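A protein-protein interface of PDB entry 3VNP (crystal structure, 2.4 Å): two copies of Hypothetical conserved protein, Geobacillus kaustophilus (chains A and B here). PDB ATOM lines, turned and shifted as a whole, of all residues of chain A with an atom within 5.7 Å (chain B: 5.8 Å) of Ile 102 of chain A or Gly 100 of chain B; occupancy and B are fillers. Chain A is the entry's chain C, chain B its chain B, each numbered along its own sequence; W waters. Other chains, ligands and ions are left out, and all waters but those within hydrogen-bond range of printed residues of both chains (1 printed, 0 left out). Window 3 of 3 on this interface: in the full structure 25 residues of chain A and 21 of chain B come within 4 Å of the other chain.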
ATOM      1  N   VAL A  84     -19.831  -4.047  -4.165  1.00  0.00           N
ATOM      2  CA  VAL A  84     -20.071  -4.810  -2.957  1.00  0.00           C
ATOM      3  C   VAL A  84     -18.932  -4.548  -1.970  1.00  0.00           C
ATOM      4  O   VAL A  84     -17.800  -4.267  -2.372  1.00  0.00           O
ATOM      5  CB  VAL A  84     -20.163  -6.320  -3.273  1.00  0.00           C
ATOM      6  CG1 VAL A  84     -20.112  -7.132  -1.988  1.00  0.00           C
ATOM      7  CG2 VAL A  84     -21.447  -6.605  -4.060  1.00  0.00           C
ATOM      8  N   ILE A  85     -19.242  -4.586  -0.682  1.00  0.00           N
ATOM      9  CA  ILE A  85     -18.216  -4.407   0.329  1.00  0.00           C
ATOM     10  C   ILE A  85     -18.045  -5.749   1.024  1.00  0.00           C
ATOM     11  O   ILE A  85     -18.990  -6.274   1.606  1.00  0.00           O
ATOM     12  CB  ILE A  85     -18.612  -3.375   1.404  1.00  0.00           C
ATOM     13  CG1 ILE A  85     -18.783  -1.994   0.781  1.00  0.00           C
ATOM     14  CG2 ILE A  85     -17.537  -3.329   2.487  1.00  0.00           C
ATOM     15  CD1 ILE A  85     -19.286  -0.949   1.767  1.00  0.00           C
ATOM     16  N   GLY A 100     -24.417  -4.086  -4.629  1.00  0.00           N
ATOM     17  CA  GLY A 100     -24.789  -3.116  -3.617  1.00  0.00           C
ATOM     18  C   GLY A 100     -24.920  -3.694  -2.226  1.00  0.00           C
ATOM     19  O   GLY A 100     -25.480  -3.050  -1.336  1.00  0.00           O
ATOM     20  N   SER A 101     -24.409  -4.904  -2.022  1.00  0.00           N
ATOM     21  CA  SER A 101     -24.497  -5.538  -0.709  1.00  0.00           C
ATOM     22  C   SER A 101     -23.250  -5.313   0.134  1.00  0.00           C
ATOM     23  O   SER A 101     -22.164  -5.057  -0.392  1.00  0.00           O
ATOM     24  CB  SER A 101     -24.724  -7.043  -0.855  1.00  0.00           C
ATOM     25  OG  SER A 101     -25.977  -7.305  -1.445  1.00  0.00           O
ATOM     26  N   ILE A 102     -23.426  -5.413   1.446  1.00  0.00           N
ATOM     27  CA  ILE A 102     -22.338  -5.260   2.404  1.00  0.00           C
ATOM     28  C   ILE A 102     -22.298  -6.541   3.238  1.00  0.00           C
ATOM     29  O   ILE A 102     -23.273  -6.882   3.914  1.00  0.00           O
ATOM     30  CB  ILE A 102     -22.578  -4.046   3.329  1.00  0.00           C
ATOM     31  CG1 ILE A 102     -22.711  -2.778   2.489  1.00  0.00           C
ATOM     32  CG2 ILE A 102     -21.433  -3.908   4.326  1.00  0.00           C
ATOM     33  CD1 ILE A 102     -23.029  -1.531   3.298  1.00  0.00           C
ATOM     34  N   ILE A 103     -21.183  -7.262   3.158  1.00  0.00           N
ATOM     35  CA  ILE A 103     -21.008  -8.509   3.896  1.00  0.00           C
ATOM     36  C   ILE A 103     -19.967  -8.243   4.977  1.00  0.00           C
ATOM     37  O   ILE A 103     -18.773  -8.116   4.683  1.00  0.00           O
ATOM     38  CB  ILE A 103     -20.485  -9.640   2.978  1.00  0.00           C
ATOM     39  CG1 ILE A 103     -21.348  -9.746   1.711  1.00  0.00           C
ATOM     40  CG2 ILE A 103     -20.452 -10.956   3.753  1.00  0.00           C
ATOM     41  CD1 ILE A 103     -22.801 -10.133   1.931  1.00  0.00           C
ATOM     42  N   LEU A 104     -20.413  -8.177   6.227  1.00  0.00           N
ATOM     43  CA  LEU A 104     -19.510  -7.871   7.330  1.00  0.00           C
ATOM     44  C   LEU A 104     -18.666  -8.997   7.947  1.00  0.00           C
ATOM     45  O   LEU A 104     -18.768 -10.175   7.596  1.00  0.00           O
ATOM     46  CB  LEU A 104     -20.279  -7.118   8.420  1.00  0.00           C
ATOM     47  CG  LEU A 104     -20.890  -5.801   7.915  1.00  0.00           C
ATOM     48  CD1 LEU A 104     -21.674  -5.118   9.027  1.00  0.00           C
ATOM     49  CD2 LEU A 104     -19.788  -4.887   7.419  1.00  0.00           C
ATOM     50  N   GLY A 118     -28.367  -5.165  -2.707  1.00  0.00           N
ATOM     51  CA  GLY A 118     -28.553  -4.182  -1.657  1.00  0.00           C
ATOM     52  C   GLY A 118     -28.667  -4.677  -0.228  1.00  0.00           C
ATOM     53  O   GLY A 118     -29.060  -3.909   0.648  1.00  0.00           O
ATOM     54  N   SER A 119     -28.308  -5.932   0.027  1.00  0.00           N
ATOM     55  CA  SER A 119     -28.405  -6.497   1.374  1.00  0.00           C
ATOM     56  C   SER A 119     -27.216  -6.224   2.294  1.00  0.00           C
ATOM     57  O   SER A 119     -26.125  -5.896   1.838  1.00  0.00           O
ATOM     58  CB  SER A 119     -28.605  -8.006   1.288  1.00  0.00           C
ATOM     59  OG  SER A 119     -29.767  -8.324   0.549  1.00  0.00           O
ATOM     60  N   LEU A 120     -27.444  -6.360   3.600  1.00  0.00           N
ATOM     61  CA  LEU A 120     -26.385  -6.177   4.589  1.00  0.00           C
ATOM     62  C   LEU A 120     -26.388  -7.406   5.497  1.00  0.00           C
ATOM     63  O   LEU A 120     -27.358  -7.647   6.219  1.00  0.00           O
ATOM     64  CB  LEU A 120     -26.603  -4.899   5.423  1.00  0.00           C
ATOM     65  CG  LEU A 120     -25.486  -4.552   6.435  1.00  0.00           C
ATOM     66  CD1 LEU A 120     -25.583  -3.103   6.897  1.00  0.00           C
ATOM     67  CD2 LEU A 120     -25.567  -5.485   7.630  1.00  0.00           C
ATOM     68  N   VAL A 121     -25.310  -8.190   5.436  1.00  0.00           N
ATOM     69  CA  VAL A 121     -25.168  -9.387   6.253  1.00  0.00           C
ATOM     70  C   VAL A 121     -24.268  -8.992   7.420  1.00  0.00           C
ATOM     71  O   VAL A 121     -23.066  -8.782   7.253  1.00  0.00           O
ATOM     72  CB  VAL A 121     -24.534 -10.542   5.439  1.00  0.00           C
ATOM     73  CG1 VAL A 121     -24.391 -11.798   6.310  1.00  0.00           C
ATOM     74  CG2 VAL A 121     -25.402 -10.840   4.208  1.00  0.00           C
ATOM     75  N   PRO A 122     -24.847  -8.892   8.624  1.00  0.00           N
ATOM     76  CA  PRO A 122     -24.137  -8.510   9.846  1.00  0.00           C
ATOM     77  C   PRO A 122     -23.030  -9.453  10.306  1.00  0.00           C
ATOM     78  O   PRO A 122     -23.000 -10.629   9.936  1.00  0.00           O
ATOM     79  CB  PRO A 122     -25.268  -8.394  10.863  1.00  0.00           C
ATOM     80  CG  PRO A 122     -26.173  -9.517  10.440  1.00  0.00           C
ATOM     81  CD  PRO A 122     -26.209  -9.362   8.938  1.00  0.00           C
ATOM     82  N   ARG A 136     -31.831  -5.943   5.212  1.00  0.00           N
ATOM     83  CA  ARG A 136     -30.860  -5.293   6.079  1.00  0.00           C
ATOM     84  C   ARG A 136     -31.431  -5.249   7.493  1.00  0.00           C
ATOM     85  O   ARG A 136     -32.255  -4.388   7.811  1.00  0.00           O
ATOM     86  CB  ARG A 136     -30.586  -3.868   5.571  1.00  0.00           C
ATOM     87  CG  ARG A 136     -30.195  -3.799   4.085  1.00  0.00           C
ATOM     88  CD  ARG A 136     -30.227  -2.375   3.539  1.00  0.00           C
ATOM     89  NE  ARG A 136     -29.118  -1.547   4.009  1.00  0.00           N
ATOM     90  CZ  ARG A 136     -27.918  -1.485   3.430  1.00  0.00           C
ATOM     91  NH1 ARG A 136     -27.645  -2.206   2.347  1.00  0.00           N
ATOM     92  NH2 ARG A 136     -26.992  -0.677   3.927  1.00  0.00           N
ATOM     93  N   GLY B  81     -15.403   5.272   6.956  1.00  0.00           N
ATOM     94  CA  GLY B  81     -15.232   4.001   6.284  1.00  0.00           C
ATOM     95  C   GLY B  81     -15.314   3.985   4.777  1.00  0.00           C
ATOM     96  O   GLY B  81     -15.623   4.996   4.141  1.00  0.00           O
ATOM     97  N   HIS B  82     -15.036   2.813   4.210  1.00  0.00           N
ATOM     98  CA  HIS B  82     -15.061   2.618   2.770  1.00  0.00           C
ATOM     99  C   HIS B  82     -16.416   2.954   2.185  1.00  0.00           C
ATOM    100  O   HIS B  82     -17.455   2.771   2.828  1.00  0.00           O
ATOM    101  CB  HIS B  82     -14.799   1.151   2.391  1.00  0.00           C
ATOM    102  CG  HIS B  82     -13.723   0.484   3.182  1.00  0.00           C
ATOM    103  ND1 HIS B  82     -12.380   0.676   2.931  1.00  0.00           N
ATOM    104  CD2 HIS B  82     -13.792  -0.402   4.202  1.00  0.00           C
ATOM    105  CE1 HIS B  82     -11.670  -0.064   3.760  1.00  0.00           C
ATOM    106  NE2 HIS B  82     -12.503  -0.729   4.542  1.00  0.00           N
ATOM    107  N   GLN B  83     -16.385   3.424   0.944  1.00  0.00           N
ATOM    108  CA  GLN B  83     -17.588   3.704   0.177  1.00  0.00           C
ATOM    109  C   GLN B  83     -18.642   4.485   0.945  1.00  0.00           C
ATOM    110  O   GLN B  83     -19.809   4.100   0.993  1.00  0.00           O
ATOM    111  CB  GLN B  83     -18.158   2.370  -0.282  1.00  0.00           C
ATOM    112  CG  GLN B  83     -19.019   2.395  -1.509  1.00  0.00           C
ATOM    113  CD  GLN B  83     -19.766   1.082  -1.668  1.00  0.00           C
ATOM    114  OE1 GLN B  83     -20.772   0.840  -0.989  1.00  0.00           O
ATOM    115  NE2 GLN B  83     -19.259   0.214  -2.540  1.00  0.00           N
ATOM    116  N   VAL B  84     -18.229   5.581   1.552  1.00  0.00           N
ATOM    117  CA  VAL B  84     -19.157   6.405   2.297  1.00  0.00           C
ATOM    118  C   VAL B  84     -19.475   7.646   1.482  1.00  0.00           C
ATOM    119  O   VAL B  84     -18.603   8.188   0.808  1.00  0.00           O
ATOM    120  CB  VAL B  84     -18.549   6.831   3.668  1.00  0.00           C
ATOM    121  CG1 VAL B  84     -19.327   8.022   4.263  1.00  0.00           C
ATOM    122  CG2 VAL B  84     -18.564   5.641   4.631  1.00  0.00           C
ATOM    123  N   GLY B  98     -19.398   4.547   9.797  1.00  0.00           N
ATOM    124  CA  GLY B  98     -19.286   3.189   9.296  1.00  0.00           C
ATOM    125  C   GLY B  98     -19.323   3.057   7.786  1.00  0.00           C
ATOM    126  O   GLY B  98     -19.988   3.839   7.099  1.00  0.00           O
ATOM    127  N   MET B  99     -18.618   2.053   7.272  1.00  0.00           N
ATOM    128  CA  MET B  99     -18.554   1.798   5.837  1.00  0.00           C
ATOM    129  C   MET B  99     -19.943   1.628   5.210  1.00  0.00           C
ATOM    130  O   MET B  99     -20.859   1.091   5.834  1.00  0.00           O
ATOM    131  CB  MET B  99     -17.703   0.548   5.565  1.00  0.00           C
ATOM    132  CG  MET B  99     -18.256  -0.736   6.175  1.00  0.00           C
ATOM    133  SD  MET B  99     -17.152  -2.158   6.011  1.00  0.00           S
ATOM    134  CE  MET B  99     -16.357  -2.152   7.649  1.00  0.00           C
ATOM    135  N   GLY B 100     -20.084   2.103   3.973  1.00  0.00           N
ATOM    136  CA  GLY B 100     -21.345   1.999   3.264  1.00  0.00           C
ATOM    137  C   GLY B 100     -22.461   2.897   3.782  1.00  0.00           C
ATOM    138  O   GLY B 100     -23.637   2.630   3.542  1.00  0.00           O
ATOM    139  N   SER B 101     -22.103   3.963   4.487  1.00  0.00           N
ATOM    140  CA  SER B 101     -23.105   4.873   5.031  1.00  0.00           C
ATOM    141  C   SER B 101     -23.289   6.116   4.174  1.00  0.00           C
ATOM    142  O   SER B 101     -22.413   6.486   3.386  1.00  0.00           O
ATOM    143  CB  SER B 101     -22.728   5.294   6.456  1.00  0.00           C
ATOM    144  OG  SER B 101     -22.680   4.177   7.329  1.00  0.00           O
ATOM    145  N   ILE B 102     -24.442   6.755   4.333  1.00  0.00           N
ATOM    146  CA  ILE B 102     -24.760   7.968   3.595  1.00  0.00           C
ATOM    147  C   ILE B 102     -25.148   9.015   4.627  1.00  0.00           C
ATOM    148  O   ILE B 102     -26.156   8.873   5.315  1.00  0.00           O
ATOM    149  CB  ILE B 102     -25.929   7.727   2.603  1.00  0.00           C
ATOM    150  CG1 ILE B 102     -25.503   6.700   1.553  1.00  0.00           C
ATOM    151  CG2 ILE B 102     -26.333   9.030   1.916  1.00  0.00           C
ATOM    152  CD1 ILE B 102     -26.626   6.246   0.637  1.00  0.00           C
ATOM    153  N   ALA B 117     -22.225   0.659  10.199  1.00  0.00           N
ATOM    154  CA  ALA B 117     -22.111   0.388   8.768  1.00  0.00           C
ATOM    155  C   ALA B 117     -23.452   0.406   8.040  1.00  0.00           C
ATOM    156  O   ALA B 117     -24.485   0.073   8.613  1.00  0.00           O
ATOM    157  CB  ALA B 117     -21.421  -0.959   8.548  1.00  0.00           C
ATOM    158  N   GLY B 118     -23.420   0.807   6.773  1.00  0.00           N
ATOM    159  CA  GLY B 118     -24.620   0.861   5.959  1.00  0.00           C
ATOM    160  C   GLY B 118     -25.751   1.753   6.435  1.00  0.00           C
ATOM    161  O   GLY B 118     -26.893   1.561   6.017  1.00  0.00           O
ATOM    162  N   SER B 119     -25.460   2.735   7.283  1.00  0.00           N
ATOM    163  CA  SER B 119     -26.516   3.613   7.792  1.00  0.00           C
ATOM    164  C   SER B 119     -26.805   4.810   6.898  1.00  0.00           C
ATOM    165  O   SER B 119     -26.045   5.119   5.982  1.00  0.00           O
ATOM    166  CB  SER B 119     -26.164   4.121   9.194  1.00  0.00           C
ATOM    167  OG  SER B 119     -26.003   3.044  10.095  1.00  0.00           O
ATOM    168  N   ARG B 136     -31.405   2.975   8.816  1.00  0.00           N
ATOM    169  CA  ARG B 136     -31.819   3.834   7.709  1.00  0.00           C
ATOM    170  C   ARG B 136     -33.313   4.120   7.823  1.00  0.00           C
ATOM    171  O   ARG B 136     -34.135   3.298   7.434  1.00  0.00           O
ATOM    172  CB  ARG B 136     -31.543   3.147   6.370  1.00  0.00           C
ATOM    173  CG  ARG B 136     -30.106   2.717   6.158  1.00  0.00           C
ATOM    174  CD  ARG B 136     -29.992   1.808   4.940  1.00  0.00           C
ATOM    175  NE  ARG B 136     -30.105   2.516   3.665  1.00  0.00           N
ATOM    176  CZ  ARG B 136     -29.071   2.983   2.966  1.00  0.00           C
ATOM    177  NH1 ARG B 136     -27.833   2.826   3.411  1.00  0.00           N
ATOM    178  NH2 ARG B 136     -29.278   3.598   1.809  1.00  0.00           N
HETATM  179  O   HOH W   1     -29.106  -0.755   7.129  1.00  0.00           O
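O of Gly 118 of chain B is in hydrogen-bond range of NH2 of Arg 136 of chain A, at 3.1 Å.
The side-chain hydroxyl (OG) of Ser 101 of chain B is in hydrogen-bond range of the backbone NH (N) of Gly 118 of chain B.
The backbone NH of Ile 85 of chain A is in hydrogen-bond range of the backbone carbonyl oxygen of Ser 101 of chain A, 3.0 Å away.
NH1 of Arg 136 of chain B is in hydrogen-bond range of O of Gly 118 of chain B (3.0 Å).
N of Ile 102 of chain A is in hydrogen-bond range of O of Ser 119 of chain A, at 2.8 Å.
NH1 of Arg 136 of chain A sits at hydrogen-bond distance from O of Gly 118 of chain A, at 2.8 Å.
The backbone carbonyl oxygen (O) of Ile 102 of chain A sits at hydrogen-bond distance from the backbone NH (N) of Val 121 of chain A, 2.9 Å away.
Ile 85 of chain A touches Gln 83 of chain B (CD1 to OE1, 3.6 Å).
Ile 85 of chain A touches Met 99 of chain B (CG2 to SD, 3.7 Å).
Ile 85 of chain A touches Gly 100 of chain B (CD1 to N, 3.8 Å).
Gly 100 of chain B touches Ile 102 of chain A.
Ile 102 of chain A touches Gly 118 of chain B.
Ala 117 of chain B touches Leu 120 of chain A (O to CD1, 3.8 Å).
Arg 136 of chain A touches Arg 136 of chain B (NE to CD, 3.6 Å).
Ile 102 of chain A touches just these residues of chain B: Gly 100 and Gly 118.
Printed residues of chain A within 4 Å of Gly 100 of chain B: Ile 85 and Ile 102.
Of the printed residues of chain A, Gly 118 of chain B touches Ile 102 and Arg 136.
Of the printed residues of chain A, Arg 136 of chain B touches Arg 136 (3.6 Å).
Ser 101 of chain B touches none of the printed residues of chain A.
Ile 103 of chain A touches none of the printed residues of chain B.
The nearest residue of chain A that does not touch Gly 100 of chain B is Arg 136 of chain A (4.7 Å).
The nearest printed residue of chain B that does not touch Ile 85 of chain A is His 82 of chain B (4.3 Å).
Of the 13 printed residues of chain B, 6 touch a printed residue of chain A.
Printed residues of chain B that touch a printed residue of chain A: Gln 83, Met 99, Gly 100, Ala 117, Gly 118 and Arg 136.
Hydrophobic or aromatic side chains of chain B that line the printed part of chain A: Met 99.
Hydrophobic or aromatic side chains of chain A that line the printed part of chain B: Ile 85, Ile 102 and Leu 120.
Ile 102 of chain A touches Gly 100 of chain B, but with the chains exchanged Gly 100 of chain A does not touch Ile 102 of chain B (9.6 Å).
Ile 102 of chain A touches Gly 118 of chain B, but with the chains exchanged Gly 118 of chain A does not touch Ile 102 of chain B (10.4 Å).
Arg 136 of chain A touches Gly 118 of chain B, but with the chains exchanged Gly 118 of chain A does not touch Arg 136 of chain B (7.2 Å).
Arg 136 of chain A touches its own counterpart, Arg 136 of chain B.
Water W1 lies within hydrogen-bond range of the guanidinium group of Arg 136 of chain A (3.2 Å) and the backbone carbonyl oxygen of Gly 118 of chain B (3.4 Å).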
